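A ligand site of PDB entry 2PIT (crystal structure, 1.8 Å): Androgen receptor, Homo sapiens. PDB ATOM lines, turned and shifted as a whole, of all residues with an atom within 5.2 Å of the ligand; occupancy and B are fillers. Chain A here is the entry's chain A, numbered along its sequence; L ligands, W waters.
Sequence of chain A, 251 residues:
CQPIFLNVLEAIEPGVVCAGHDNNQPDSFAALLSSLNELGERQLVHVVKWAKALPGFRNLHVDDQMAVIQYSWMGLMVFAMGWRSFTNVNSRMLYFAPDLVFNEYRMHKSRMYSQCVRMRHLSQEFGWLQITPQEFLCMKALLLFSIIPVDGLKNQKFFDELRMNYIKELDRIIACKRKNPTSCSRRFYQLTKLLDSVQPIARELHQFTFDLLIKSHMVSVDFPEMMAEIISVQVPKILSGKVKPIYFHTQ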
ATOM      1  N   LEU A  33       9.744  11.208  -4.405  1.00  0.00           N
ATOM      2  CA  LEU A  33       9.167  10.988  -3.084  1.00  0.00           C
ATOM      3  C   LEU A  33      10.031  11.556  -1.965  1.00  0.00           C
ATOM      4  O   LEU A  33       9.510  12.104  -0.996  1.00  0.00           O
ATOM      5  CB  LEU A  33       8.881   9.499  -2.858  1.00  0.00           C
ATOM      6  CG  LEU A  33       7.476   9.057  -3.272  1.00  0.00           C
ATOM      7  CD1 LEU A  33       6.436   9.761  -2.390  1.00  0.00           C
ATOM      8  CD2 LEU A  33       7.236   9.393  -4.745  1.00  0.00           C
ATOM      9  N   LEU A  36       9.322  15.099  -1.900  1.00  0.00           N
ATOM     10  CA  LEU A  36       7.984  15.346  -1.339  1.00  0.00           C
ATOM     11  C   LEU A  36       8.054  15.222   0.180  1.00  0.00           C
ATOM     12  O   LEU A  36       7.425  16.005   0.903  1.00  0.00           O
ATOM     13  CB  LEU A  36       6.952  14.353  -1.889  1.00  0.00           C
ATOM     14  CG  LEU A  36       6.337  14.658  -3.277  1.00  0.00           C
ATOM     15  CD1 LEU A  36       5.414  13.539  -3.695  1.00  0.00           C
ATOM     16  CD2 LEU A  36       5.558  15.976  -3.206  1.00  0.00           C
ATOM     17  N   ASN A  37       8.826  14.254   0.660  1.00  0.00           N
ATOM     18  CA  ASN A  37       8.979  14.063   2.109  1.00  0.00           C
ATOM     19  C   ASN A  37       9.698  15.236   2.751  1.00  0.00           C
ATOM     20  O   ASN A  37       9.333  15.680   3.840  1.00  0.00           O
ATOM     21  CB  ASN A  37       9.742  12.769   2.403  1.00  0.00           C
ATOM     22  CG  ASN A  37       8.871  11.531   2.223  1.00  0.00           C
ATOM     23  OD1 ASN A  37       7.654  11.614   2.308  1.00  0.00           O
ATOM     24  ND2 ASN A  37       9.509  10.388   2.014  1.00  0.00           N
ATOM     25  N   LEU A  39       9.727  18.230   1.549  1.00  0.00           N
ATOM     26  CA  LEU A  39       8.781  19.328   1.468  1.00  0.00           C
ATOM     27  C   LEU A  39       7.815  19.237   2.651  1.00  0.00           C
ATOM     28  O   LEU A  39       7.473  20.247   3.273  1.00  0.00           O
ATOM     29  CB  LEU A  39       7.983  19.280   0.156  1.00  0.00           C
ATOM     30  CG  LEU A  39       6.896  20.352   0.023  1.00  0.00           C
ATOM     31  CD1 LEU A  39       7.525  21.739   0.198  1.00  0.00           C
ATOM     32  CD2 LEU A  39       6.210  20.261  -1.335  1.00  0.00           C
ATOM     33  N   GLY A  40       7.362  18.030   2.931  1.00  0.00           N
ATOM     34  CA  GLY A  40       6.446  17.829   4.043  1.00  0.00           C
ATOM     35  C   GLY A  40       7.040  18.283   5.364  1.00  0.00           C
ATOM     36  O   GLY A  40       6.368  18.927   6.174  1.00  0.00           O
ATOM     37  N   GLN A  43       7.246  22.114   5.323  1.00  0.00           N
ATOM     38  CA  GLN A  43       5.914  22.661   5.477  1.00  0.00           C
ATOM     39  C   GLN A  43       5.380  22.467   6.892  1.00  0.00           C
ATOM     40  O   GLN A  43       4.648  23.306   7.402  1.00  0.00           O
ATOM     41  CB  GLN A  43       4.958  22.005   4.485  1.00  0.00           C
ATOM     42  CG  GLN A  43       5.032  22.593   3.086  1.00  0.00           C
ATOM     43  CD  GLN A  43       4.382  23.961   3.005  1.00  0.00           C
ATOM     44  OE1 GLN A  43       4.417  24.631   1.957  1.00  0.00           O
ATOM     45  NE2 GLN A  43       3.762  24.391   4.099  1.00  0.00           N
ATOM     46  N   TRP A  73      -2.185  17.593   9.687  1.00  0.00           N
ATOM     47  CA  TRP A  73      -1.254  18.133   8.709  1.00  0.00           C
ATOM     48  C   TRP A  73      -1.438  17.683   7.264  1.00  0.00           C
ATOM     49  O   TRP A  73      -1.279  18.471   6.333  1.00  0.00           O
ATOM     50  CB  TRP A  73       0.206  17.873   9.125  1.00  0.00           C
ATOM     51  CG  TRP A  73       0.587  16.433   9.210  1.00  0.00           C
ATOM     52  CD1 TRP A  73       0.441  15.612  10.291  1.00  0.00           C
ATOM     53  CD2 TRP A  73       1.161  15.629   8.178  1.00  0.00           C
ATOM     54  NE1 TRP A  73       0.885  14.344   9.990  1.00  0.00           N
ATOM     55  CE2 TRP A  73       1.330  14.326   8.699  1.00  0.00           C
ATOM     56  CE3 TRP A  73       1.547  15.884   6.847  1.00  0.00           C
ATOM     57  CZ2 TRP A  73       1.874  13.277   7.939  1.00  0.00           C
ATOM     58  CZ3 TRP A  73       2.087  14.835   6.096  1.00  0.00           C
ATOM     59  CH2 TRP A  73       2.242  13.543   6.654  1.00  0.00           C
ATOM     60  N   MET A  74      -1.758  16.413   7.048  1.00  0.00           N
ATOM     61  CA  MET A  74      -1.931  15.935   5.686  1.00  0.00           C
ATOM     62  C   MET A  74      -3.067  16.661   4.977  1.00  0.00           C
ATOM     63  O   MET A  74      -2.898  17.170   3.866  1.00  0.00           O
ATOM     64  CB  MET A  74      -2.185  14.411   5.676  1.00  0.00           C
ATOM     65  CG  MET A  74      -2.318  13.813   4.283  1.00  0.00           C
ATOM     66  SD  MET A  74      -0.740  13.733   3.416  1.00  0.00           S
ATOM     67  CE  MET A  74      -0.045  12.254   4.171  1.00  0.00           C
ATOM     68  N   MET A  77      -2.170  20.406   4.372  1.00  0.00           N
ATOM     69  CA  MET A  77      -1.198  20.581   3.297  1.00  0.00           C
ATOM     70  C   MET A  77      -1.745  20.284   1.913  1.00  0.00           C
ATOM     71  O   MET A  77      -1.402  20.960   0.938  1.00  0.00           O
ATOM     72  CB  MET A  77       0.033  19.716   3.551  1.00  0.00           C
ATOM     73  CG  MET A  77       0.814  20.141   4.793  1.00  0.00           C
ATOM     74  SD  MET A  77       2.299  19.182   4.935  1.00  0.00           S
ATOM     75  CE  MET A  77       2.936  19.733   6.535  1.00  0.00           C
ATOM     76  N   VAL A  78      -2.585  19.262   1.813  1.00  0.00           N
ATOM     77  CA  VAL A  78      -3.188  18.899   0.538  1.00  0.00           C
ATOM     78  C   VAL A  78      -4.155  19.993   0.085  1.00  0.00           C
ATOM     79  O   VAL A  78      -4.211  20.351  -1.088  1.00  0.00           O
ATOM     80  CB  VAL A  78      -3.942  17.557   0.634  1.00  0.00           C
ATOM     81  CG1 VAL A  78      -4.763  17.316  -0.613  1.00  0.00           C
ATOM     82  CG2 VAL A  78      -2.940  16.418   0.842  1.00  0.00           C
ATOM     83  N   MET A  81      -2.235  22.934  -1.054  1.00  0.00           N
ATOM     84  CA  MET A  81      -1.610  22.596  -2.327  1.00  0.00           C
ATOM     85  C   MET A  81      -2.635  22.703  -3.452  1.00  0.00           C
ATOM     86  O   MET A  81      -2.333  23.190  -4.545  1.00  0.00           O
ATOM     87  CB  MET A  81      -1.038  21.175  -2.278  1.00  0.00           C
ATOM     88  CG  MET A  81      -0.214  20.777  -3.502  1.00  0.00           C
ATOM     89  SD  MET A  81      -1.216  20.195  -4.891  1.00  0.00           S
ATOM     90  CE  MET A  81      -1.686  18.552  -4.280  1.00  0.00           C
ATOM     91  N   ARG A  84      -2.962  26.331  -4.240  1.00  0.00           N
ATOM     92  CA  ARG A  84      -1.796  26.833  -4.990  1.00  0.00           C
ATOM     93  C   ARG A  84      -1.856  26.407  -6.445  1.00  0.00           C
ATOM     94  O   ARG A  84      -1.489  27.176  -7.348  1.00  0.00           O
ATOM     95  CB  ARG A  84      -0.486  26.270  -4.418  1.00  0.00           C
ATOM     96  CG  ARG A  84      -0.047  26.833  -3.116  1.00  0.00           C
ATOM     97  CD  ARG A  84       1.444  26.568  -2.916  1.00  0.00           C
ATOM     98  NE  ARG A  84       1.738  25.153  -2.729  1.00  0.00           N
ATOM     99  CZ  ARG A  84       1.438  24.460  -1.635  1.00  0.00           C
ATOM    100  NH1 ARG A  84       0.821  25.059  -0.624  1.00  0.00           N
ATOM    101  NH2 ARG A  84       1.785  23.191  -1.530  1.00  0.00           N
ATOM    102  N   PHE A  96       3.070  21.489  -5.877  1.00  0.00           N
ATOM    103  CA  PHE A  96       3.516  21.193  -4.510  1.00  0.00           C
ATOM    104  C   PHE A  96       4.428  22.310  -4.021  1.00  0.00           C
ATOM    105  O   PHE A  96       4.271  22.796  -2.895  1.00  0.00           O
ATOM    106  CB  PHE A  96       4.254  19.858  -4.479  1.00  0.00           C
ATOM    107  CG  PHE A  96       3.364  18.671  -4.736  1.00  0.00           C
ATOM    108  CD1 PHE A  96       2.453  18.261  -3.777  1.00  0.00           C
ATOM    109  CD2 PHE A  96       3.454  17.969  -5.936  1.00  0.00           C
ATOM    110  CE1 PHE A  96       1.627  17.150  -4.008  1.00  0.00           C
ATOM    111  CE2 PHE A  96       2.635  16.867  -6.176  1.00  0.00           C
ATOM    112  CZ  PHE A  96       1.719  16.458  -5.208  1.00  0.00           C
ATOM    113  N   MET A 112       1.848   7.180  -7.450  1.00  0.00           N
ATOM    114  CA  MET A 112       0.627   7.524  -6.720  1.00  0.00           C
ATOM    115  C   MET A 112      -0.225   8.353  -7.669  1.00  0.00           C
ATOM    116  O   MET A 112      -0.737   9.417  -7.312  1.00  0.00           O
ATOM    117  CB  MET A 112       0.923   8.285  -5.416  1.00  0.00           C
ATOM    118  CG  MET A 112       1.892   9.444  -5.517  1.00  0.00           C
ATOM    119  SD  MET A 112       2.035  10.263  -3.899  1.00  0.00           S
ATOM    120  CE  MET A 112       0.850  11.578  -4.098  1.00  0.00           C
ATOM    121  N   MET A 119      -6.350  14.560  -5.972  1.00  0.00           N
ATOM    122  CA  MET A 119      -5.828  15.853  -5.545  1.00  0.00           C
ATOM    123  C   MET A 119      -6.026  16.918  -6.628  1.00  0.00           C
ATOM    124  O   MET A 119      -6.333  18.062  -6.325  1.00  0.00           O
ATOM    125  CB  MET A 119      -4.348  15.766  -5.172  1.00  0.00           C
ATOM    126  CG  MET A 119      -4.074  14.981  -3.903  1.00  0.00           C
ATOM    127  SD  MET A 119      -2.431  15.292  -3.245  1.00  0.00           S
ATOM    128  CE  MET A 119      -1.449  14.175  -4.233  1.00  0.00           C
ATOM    129  N   LEU A 205      -3.594   9.135   1.216  1.00  0.00           N
ATOM    130  CA  LEU A 205      -2.205   9.548   1.306  1.00  0.00           C
ATOM    131  C   LEU A 205      -1.571   9.008   2.593  1.00  0.00           C
ATOM    132  O   LEU A 205      -0.396   8.641   2.612  1.00  0.00           O
ATOM    133  CB  LEU A 205      -2.096  11.079   1.240  1.00  0.00           C
ATOM    134  CG  LEU A 205      -2.361  11.703  -0.138  1.00  0.00           C
ATOM    135  CD1 LEU A 205      -2.212  13.217  -0.054  1.00  0.00           C
ATOM    136  CD2 LEU A 205      -1.386  11.146  -1.166  1.00  0.00           C
ATOM    137  N   PHE A 208      -0.745   5.467   1.835  1.00  0.00           N
ATOM    138  CA  PHE A 208       0.403   5.417   0.938  1.00  0.00           C
ATOM    139  C   PHE A 208       1.724   5.759   1.626  1.00  0.00           C
ATOM    140  O   PHE A 208       2.735   5.072   1.454  1.00  0.00           O
ATOM    141  CB  PHE A 208       0.177   6.340  -0.261  1.00  0.00           C
ATOM    142  CG  PHE A 208       1.260   6.272  -1.296  1.00  0.00           C
ATOM    143  CD1 PHE A 208       2.406   7.059  -1.179  1.00  0.00           C
ATOM    144  CD2 PHE A 208       1.152   5.404  -2.380  1.00  0.00           C
ATOM    145  CE1 PHE A 208       3.432   6.989  -2.141  1.00  0.00           C
ATOM    146  CE2 PHE A 208       2.164   5.317  -3.347  1.00  0.00           C
ATOM    147  CZ  PHE A 208       3.308   6.114  -3.221  1.00  0.00           C
ATOM    148  N   THR A 209       1.743   6.831   2.407  1.00  0.00           N
ATOM    149  CA  THR A 209       2.989   7.213   3.059  1.00  0.00           C
ATOM    150  C   THR A 209       3.391   6.185   4.111  1.00  0.00           C
ATOM    151  O   THR A 209       4.589   5.907   4.301  1.00  0.00           O
ATOM    152  CB  THR A 209       2.899   8.628   3.678  1.00  0.00           C
ATOM    153  OG1 THR A 209       4.222   9.097   3.943  1.00  0.00           O
ATOM    154  CG2 THR A 209       2.101   8.624   4.987  1.00  0.00           C
ATOM    155  N   LEU A 212       4.962   3.342   2.350  1.00  0.00           N
ATOM    156  CA  LEU A 212       6.233   3.798   1.814  1.00  0.00           C
ATOM    157  C   LEU A 212       7.285   3.829   2.911  1.00  0.00           C
ATOM    158  O   LEU A 212       8.433   3.452   2.688  1.00  0.00           O
ATOM    159  CB  LEU A 212       6.079   5.186   1.186  1.00  0.00           C
ATOM    160  CG  LEU A 212       7.344   5.771   0.564  1.00  0.00           C
ATOM    161  CD1 LEU A 212       7.966   4.768  -0.415  1.00  0.00           C
ATOM    162  CD2 LEU A 212       7.012   7.082  -0.140  1.00  0.00           C
ATOM    163  N   PHE A 223      13.100   9.705   4.561  1.00  0.00           N
ATOM    164  CA  PHE A 223      12.086  10.377   5.369  1.00  0.00           C
ATOM    165  C   PHE A 223      12.784  11.192   6.446  1.00  0.00           C
ATOM    166  O   PHE A 223      13.538  10.641   7.250  1.00  0.00           O
ATOM    167  CB  PHE A 223      11.164   9.369   6.066  1.00  0.00           C
ATOM    168  CG  PHE A 223      10.077   8.818   5.196  1.00  0.00           C
ATOM    169  CD1 PHE A 223      10.337   7.802   4.285  1.00  0.00           C
ATOM    170  CD2 PHE A 223       8.766   9.290   5.309  1.00  0.00           C
ATOM    171  CE1 PHE A 223       9.309   7.253   3.508  1.00  0.00           C
ATOM    172  CE2 PHE A 223       7.748   8.758   4.546  1.00  0.00           C
ATOM    173  CZ  PHE A 223       8.014   7.731   3.639  1.00  0.00           C
ATOM    174  N   ILE A 231       4.678   9.620  11.039  1.00  0.00           N
ATOM    175  CA  ILE A 231       4.072   8.595  10.210  1.00  0.00           C
ATOM    176  C   ILE A 231       4.102   7.204  10.859  1.00  0.00           C
ATOM    177  O   ILE A 231       3.288   6.343  10.522  1.00  0.00           O
ATOM    178  CB  ILE A 231       4.760   8.577   8.830  1.00  0.00           C
ATOM    179  CG1 ILE A 231       4.494   9.913   8.122  1.00  0.00           C
ATOM    180  CG2 ILE A 231       4.249   7.408   7.985  1.00  0.00           C
ATOM    181  CD1 ILE A 231       5.206  10.082   6.799  1.00  0.00           C
HETATM  182  C1  LIG L   1       3.809  17.827   0.958  1.00  0.00           C
HETATM  183  C2  LIG L   1       3.211  19.244   1.085  1.00  0.00           C
HETATM  184  C3  LIG L   1       2.157  19.390  -0.055  1.00  0.00           C
HETATM  185  O1  LIG L   1       2.201  20.377  -0.773  1.00  0.00           O
HETATM  186  C4  LIG L   1       1.140  18.309  -0.221  1.00  0.00           C
HETATM  187  C5  LIG L   1       1.812  16.908  -0.380  1.00  0.00           C
HETATM  188  C6  LIG L   1       0.775  15.760  -0.541  1.00  0.00           C
HETATM  189  C7  LIG L   1       1.506  14.418  -0.720  1.00  0.00           C
HETATM  190  C8  LIG L   1       2.461  14.086   0.482  1.00  0.00           C
HETATM  191  C9  LIG L   1       3.486  15.257   0.658  1.00  0.00           C
HETATM  192  C10 LIG L   1       2.784  16.661   0.881  1.00  0.00           C
HETATM  193  C11 LIG L   1       4.450  14.892   1.844  1.00  0.00           C
HETATM  194  C12 LIG L   1       5.173  13.559   1.738  1.00  0.00           C
HETATM  195  C13 LIG L   1       4.209  12.381   1.425  1.00  0.00           C
HETATM  196  C14 LIG L   1       3.247  12.775   0.250  1.00  0.00           C
HETATM  197  C15 LIG L   1       2.439  11.474   0.046  1.00  0.00           C
HETATM  198  C16 LIG L   1       3.546  10.387   0.177  1.00  0.00           C
HETATM  199  C17 LIG L   1       4.766  11.127   0.790  1.00  0.00           C
HETATM  200  O2  LIG L   1       5.426  10.262   1.720  1.00  0.00           O
HETATM  201  C18 LIG L   1       3.396  12.031   2.744  1.00  0.00           C
HETATM  202  C19 LIG L   1       1.935  16.606   2.224  1.00  0.00           C
HETATM  203  O   HOH W   1       0.717  22.624   1.177  1.00  0.00           O
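The side-chain amide oxygen (OD1) of Asn 37 lies within hydrogen-bond range of an oxygen (O2) of the ligand, at 2.7 Å. The side-chain hydroxyl (OG1) of Thr 209 lies within hydrogen-bond range of an oxygen (O2) of the ligand (2.8 Å). An oxygen (O1) of the ligand sits at hydrogen-bond distance from the guanidinium group (NH2) of Arg 84, at 2.9 Å.
ND2 of Asn 37 lies close to O of Leu 33. The backbone carbonyl oxygen (O) of Phe 96 lies within hydrogen-bond range of the guanidinium group (NH2) of Arg 84 (2.9 Å).
Leu 33 touches the ligand (CD1 to C17, 3.8 Å). Leu 36 touches the ligand (O to C11, 3.3 Å). Leu 39 touches the ligand. CE of Met 74 touches C18 of the ligand, at 3.7 Å. Met 77 touches the ligand. CB of Met 81 touches O1 of the ligand, 3.7 Å away. Phe 96 touches the ligand. Leu 205 touches the ligand (CD1 to C6, 3.95 Å). Phe 208 touches the ligand. Phe 223 touches the ligand. Hydrophobic or aromatic side chains within 4 Å of the ligand: Leu 33, Leu 39, Met 74, Met 77, Met 81, Phe 96, Leu 205, Phe 208 and Phe 223. Within 4 Å of the ligand: Leu 33, Leu 36, Asn 37, Leu 39, Met 74, Met 77, Met 81, Arg 84, Phe 96, Leu 205, Phe 208, Thr 209 and Phe 223. Along chain A the residues within 4 Å of the ligand span positions 33 to 223. The nearest printed residue that does not touch the ligand is Leu 212 (4.01 Å).
Water W1 lies within hydrogen-bond range of the backbone carbonyl oxygen of Met 77 (2.7 Å), the guanidinium group of Arg 84 (3.0 Å) and an oxygen (O1) of the ligand (3.3 Å).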
